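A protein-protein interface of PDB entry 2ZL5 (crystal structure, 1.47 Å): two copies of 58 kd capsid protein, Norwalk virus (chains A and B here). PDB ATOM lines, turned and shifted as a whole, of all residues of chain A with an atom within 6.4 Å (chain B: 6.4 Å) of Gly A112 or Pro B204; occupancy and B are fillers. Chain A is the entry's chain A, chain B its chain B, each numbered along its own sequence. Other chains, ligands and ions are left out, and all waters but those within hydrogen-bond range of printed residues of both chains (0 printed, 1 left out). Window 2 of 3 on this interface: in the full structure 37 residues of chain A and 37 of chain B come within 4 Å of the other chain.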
ATOM      1  N   GLN A 110      21.500  13.491 -11.784  1.00  0.00           N
ATOM      2  CA  GLN A 110      22.193  13.753 -13.044  1.00  0.00           C
ATOM      3  C   GLN A 110      23.165  14.912 -12.903  1.00  0.00           C
ATOM      4  O   GLN A 110      22.835  15.955 -12.310  1.00  0.00           O
ATOM      5  CB  GLN A 110      21.177  14.137 -14.126  1.00  0.00           C
ATOM      6  CG  GLN A 110      20.193  13.055 -14.430  1.00  0.00           C
ATOM      7  CD  GLN A 110      19.254  13.456 -15.547  1.00  0.00           C
ATOM      8  OE1 GLN A 110      18.295  14.196 -15.320  1.00  0.00           O
ATOM      9  NE2 GLN A 110      19.526  12.968 -16.752  1.00  0.00           N
ATOM     10  N   PHE A 111      24.362  14.759 -13.456  1.00  0.00           N
ATOM     11  CA  PHE A 111      25.283  15.878 -13.535  1.00  0.00           C
ATOM     12  C   PHE A 111      24.737  16.904 -14.513  1.00  0.00           C
ATOM     13  O   PHE A 111      24.385  16.565 -15.647  1.00  0.00           O
ATOM     14  CB  PHE A 111      26.672  15.411 -13.963  1.00  0.00           C
ATOM     15  CG  PHE A 111      27.267  14.372 -13.038  1.00  0.00           C
ATOM     16  CD1 PHE A 111      27.540  14.677 -11.705  1.00  0.00           C
ATOM     17  CD2 PHE A 111      27.520  13.084 -13.494  1.00  0.00           C
ATOM     18  CE1 PHE A 111      28.057  13.692 -10.842  1.00  0.00           C
ATOM     19  CE2 PHE A 111      28.053  12.117 -12.645  1.00  0.00           C
ATOM     20  CZ  PHE A 111      28.322  12.435 -11.314  1.00  0.00           C
ATOM     21  N   GLY A 112      24.606  18.137 -14.032  1.00  0.00           N
ATOM     22  CA  GLY A 112      24.140  19.255 -14.863  1.00  0.00           C
ATOM     23  C   GLY A 112      22.636  19.444 -14.930  1.00  0.00           C
ATOM     24  O   GLY A 112      22.166  20.342 -15.631  1.00  0.00           O
ATOM     25  N   HIS A 113      21.866  18.623 -14.219  1.00  0.00           N
ATOM     26  CA  HIS A 113      20.400  18.730 -14.187  1.00  0.00           C
ATOM     27  C   HIS A 113      19.890  18.790 -12.760  1.00  0.00           C
ATOM     28  O   HIS A 113      20.458  18.154 -11.861  1.00  0.00           O
ATOM     29  CB  HIS A 113      19.728  17.533 -14.860  1.00  0.00           C
ATOM     30  CG  HIS A 113      20.013  17.428 -16.324  1.00  0.00           C
ATOM     31  ND1 HIS A 113      21.158  16.835 -16.816  1.00  0.00           N
ATOM     32  CD2 HIS A 113      19.306  17.839 -17.403  1.00  0.00           C
ATOM     33  CE1 HIS A 113      21.145  16.891 -18.138  1.00  0.00           C
ATOM     34  NE2 HIS A 113      20.037  17.500 -18.518  1.00  0.00           N
ATOM     35  N   SER A 114      18.813  19.531 -12.553  1.00  0.00           N
ATOM     36  CA  SER A 114      18.116  19.495 -11.280  1.00  0.00           C
ATOM     37  C   SER A 114      17.404  18.161 -11.117  1.00  0.00           C
ATOM     38  O   SER A 114      17.263  17.383 -12.069  1.00  0.00           O
ATOM     39  CB  SER A 114      17.075  20.623 -11.220  1.00  0.00           C
ATOM     40  OG  SER A 114      17.689  21.895 -11.252  1.00  0.00           O
ATOM     41  N   SER A 115      16.968  17.911  -9.882  1.00  0.00           N
ATOM     42  CA  SER A 115      15.965  16.895  -9.550  1.00  0.00           C
ATOM     43  C   SER A 115      16.543  15.512  -9.279  1.00  0.00           C
ATOM     44  O   SER A 115      17.657  15.190  -9.696  1.00  0.00           O
ATOM     45  CB  SER A 115      14.883  16.809 -10.627  1.00  0.00           C
ATOM     46  OG  SER A 115      14.304  18.079 -10.836  1.00  0.00           O
ATOM     47  N   TRP B 151      21.523  16.153  -4.171  1.00  0.00           N
ATOM     48  CA  TRP B 151      21.963  17.108  -5.186  1.00  0.00           C
ATOM     49  C   TRP B 151      21.846  18.513  -4.614  1.00  0.00           C
ATOM     50  O   TRP B 151      21.258  18.704  -3.563  1.00  0.00           O
ATOM     51  CB  TRP B 151      21.170  16.937  -6.514  1.00  0.00           C
ATOM     52  CG  TRP B 151      19.683  17.129  -6.403  1.00  0.00           C
ATOM     53  CD1 TRP B 151      18.782  16.231  -5.930  1.00  0.00           C
ATOM     54  CD2 TRP B 151      18.943  18.282  -6.808  1.00  0.00           C
ATOM     55  NE1 TRP B 151      17.507  16.761  -5.983  1.00  0.00           N
ATOM     56  CE2 TRP B 151      17.582  18.020  -6.524  1.00  0.00           C
ATOM     57  CE3 TRP B 151      19.303  19.521  -7.364  1.00  0.00           C
ATOM     58  CZ2 TRP B 151      16.567  18.941  -6.800  1.00  0.00           C
ATOM     59  CZ3 TRP B 151      18.277  20.457  -7.622  1.00  0.00           C
ATOM     60  CH2 TRP B 151      16.938  20.155  -7.326  1.00  0.00           C
ATOM     61  N   ILE B 152      22.474  19.473  -5.273  1.00  0.00           N
ATOM     62  CA  ILE B 152      22.466  20.847  -4.809  1.00  0.00           C
ATOM     63  C   ILE B 152      22.016  21.782  -5.926  1.00  0.00           C
ATOM     64  O   ILE B 152      21.974  21.389  -7.095  1.00  0.00           O
ATOM     65  CB  ILE B 152      23.843  21.310  -4.282  1.00  0.00           C
ATOM     66  CG1 ILE B 152      24.859  21.420  -5.427  1.00  0.00           C
ATOM     67  CG2 ILE B 152      24.316  20.385  -3.118  1.00  0.00           C
ATOM     68  CD1 ILE B 152      26.166  21.935  -5.002  1.00  0.00           C
ATOM     69  N   SER B 153      21.711  23.024  -5.532  1.00  0.00           N
ATOM     70  CA  SER B 153      21.325  24.078  -6.481  1.00  0.00           C
ATOM     71  C   SER B 153      21.761  25.415  -5.893  1.00  0.00           C
ATOM     72  O   SER B 153      22.224  25.484  -4.749  1.00  0.00           O
ATOM     73  CB  SER B 153      19.821  24.025  -6.731  1.00  0.00           C
ATOM     74  OG  SER B 153      19.091  24.215  -5.528  1.00  0.00           O
ATOM     75  N   PRO B 154      21.665  26.506  -6.677  1.00  0.00           N
ATOM     76  CA  PRO B 154      22.075  27.812  -6.168  1.00  0.00           C
ATOM     77  C   PRO B 154      21.341  28.211  -4.878  1.00  0.00           C
ATOM     78  O   PRO B 154      20.205  27.791  -4.680  1.00  0.00           O
ATOM     79  CB  PRO B 154      21.700  28.764  -7.329  1.00  0.00           C
ATOM     80  CG  PRO B 154      21.870  27.899  -8.529  1.00  0.00           C
ATOM     81  CD  PRO B 154      21.232  26.590  -8.094  1.00  0.00           C
ATOM     82  N   MET B 201      29.403  17.062  -8.210  1.00  0.00           N
ATOM     83  CA  MET B 201      28.163  16.980  -7.432  1.00  0.00           C
ATOM     84  C   MET B 201      26.970  17.204  -8.358  1.00  0.00           C
ATOM     85  O   MET B 201      26.941  18.213  -9.070  1.00  0.00           O
ATOM     86  CB  MET B 201      28.176  18.066  -6.351  1.00  0.00           C
ATOM     87  CG  MET B 201      26.804  18.314  -5.681  1.00  0.00           C
ATOM     88  SD  MET B 201      26.170  16.900  -4.703  1.00  0.00           S
ATOM     89  CE  MET B 201      27.157  17.140  -3.230  1.00  0.00           C
ATOM     90  N   PRO B 202      25.983  16.290  -8.366  1.00  0.00           N
ATOM     91  CA  PRO B 202      24.812  16.536  -9.219  1.00  0.00           C
ATOM     92  C   PRO B 202      24.025  17.793  -8.871  1.00  0.00           C
ATOM     93  O   PRO B 202      24.079  18.285  -7.742  1.00  0.00           O
ATOM     94  CB  PRO B 202      23.927  15.304  -9.018  1.00  0.00           C
ATOM     95  CG  PRO B 202      24.512  14.534  -7.968  1.00  0.00           C
ATOM     96  CD  PRO B 202      25.909  14.983  -7.678  1.00  0.00           C
ATOM     97  N   GLY B 203      23.278  18.278  -9.864  1.00  0.00           N
ATOM     98  CA  GLY B 203      22.535  19.529  -9.763  1.00  0.00           C
ATOM     99  C   GLY B 203      22.670  20.312 -11.063  1.00  0.00           C
ATOM    100  O   GLY B 203      23.438  19.907 -11.943  1.00  0.00           O
ATOM    101  N   PRO B 204      21.911  21.418 -11.199  1.00  0.00           N
ATOM    102  CA  PRO B 204      21.827  22.174 -12.469  1.00  0.00           C
ATOM    103  C   PRO B 204      23.037  23.064 -12.764  1.00  0.00           C
ATOM    104  O   PRO B 204      22.882  24.230 -13.119  1.00  0.00           O
ATOM    105  CB  PRO B 204      20.567  23.015 -12.275  1.00  0.00           C
ATOM    106  CG  PRO B 204      20.561  23.292 -10.782  1.00  0.00           C
ATOM    107  CD  PRO B 204      21.018  21.989 -10.164  1.00  0.00           C
ATOM    108  N   GLY B 205      24.234  22.521 -12.635  1.00  0.00           N
ATOM    109  CA  GLY B 205      25.451  23.234 -12.985  1.00  0.00           C
ATOM    110  C   GLY B 205      26.648  22.316 -12.883  1.00  0.00           C
ATOM    111  O   GLY B 205      26.506  21.149 -12.489  1.00  0.00           O
ATOM    112  N   ALA B 206      27.810  22.820 -13.282  1.00  0.00           N
ATOM    113  CA  ALA B 206      29.030  22.040 -13.283  1.00  0.00           C
ATOM    114  C   ALA B 206      29.667  22.166 -11.916  1.00  0.00           C
ATOM    115  O   ALA B 206      30.667  22.843 -11.736  1.00  0.00           O
ATOM    116  CB  ALA B 206      29.993  22.555 -14.376  1.00  0.00           C
ATOM    117  N   TYR B 207      29.058  21.518 -10.928  1.00  0.00           N
ATOM    118  CA  TYR B 207      29.494  21.700  -9.544  1.00  0.00           C
ATOM    119  C   TYR B 207      30.598  20.756  -9.129  1.00  0.00           C
ATOM    120  O   TYR B 207      30.540  19.546  -9.420  1.00  0.00           O
ATOM    121  CB  TYR B 207      28.311  21.497  -8.594  1.00  0.00           C
ATOM    122  CG  TYR B 207      27.099  22.353  -8.913  1.00  0.00           C
ATOM    123  CD1 TYR B 207      27.239  23.688  -9.316  1.00  0.00           C
ATOM    124  CD2 TYR B 207      25.818  21.833  -8.792  1.00  0.00           C
ATOM    125  CE1 TYR B 207      26.112  24.479  -9.594  1.00  0.00           C
ATOM    126  CE2 TYR B 207      24.706  22.602  -9.051  1.00  0.00           C
ATOM    127  CZ  TYR B 207      24.856  23.936  -9.462  1.00  0.00           C
ATOM    128  OH  TYR B 207      23.721  24.695  -9.738  1.00  0.00           O
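N of Ile B152 is in hydrogen-bond range of O of Pro B202 (3.2 Å). The backbone carbonyl oxygen (O) of Phe A111 lies within hydrogen-bond range of a ring nitrogen (ND1) of His A113 (3.4 Å).
Among the printed residues, merely in contact across the chains: Ser A114 with Pro B204, Ser A115 with Trp B151, Gln A110 with Pro B202, His A113 with Pro B204, Gly A112 with Pro B204, Ser A114 with Trp B151 and Gly A112 with Gly B205.
No position is printed for both chains. Of the 10 pairs that touch across the chains among the printed residues, none has its exchanged pair printed and touching as well.
Printed residues of chain A that touch a printed residue of chain B: Gln A110, Gly A112, His A113, Ser A114 and Ser A115. Among the printed residues, no Asp or Glu carboxylate lies within 4 Å of a Lys or Arg side-chain nitrogen of the other chain.
O of Gln A110 sits at hydrogen-bond distance from N of Gly B203, at 3.4 Å. The backbone NH (N) of His A113 lies within hydrogen-bond range of the backbone carbonyl oxygen (O) of Gly B203. N of Gly A112 sits at hydrogen-bond distance from O of Gly B203 (3.0 Å).
Of chain B, only Gly B203, Pro B204 and Gly B205 come within 4 Å of Gly A112. Printed residues of chain A within 4 Å of Pro B204: Gly A112 (3.7 Å), His A113 (3.6 Å) and Ser A114 (3.2 Å). Of the printed residues of chain A, Pro B202 touches Gln A110. Printed residues of chain B within 4 Å of Gln A110: Pro B202 (3.5 Å) and Gly B203 (3.4 Å). Ser B153 touches none of the printed residues of chain A. Ile B152 touches none of the printed residues of chain A. The nearest residue of chain B that does not touch Gly A112 is Pro B202 (5.1 Å). The nearest printed residue of chain A that does not touch Pro B202 is Phe A111 (4.02 Å).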
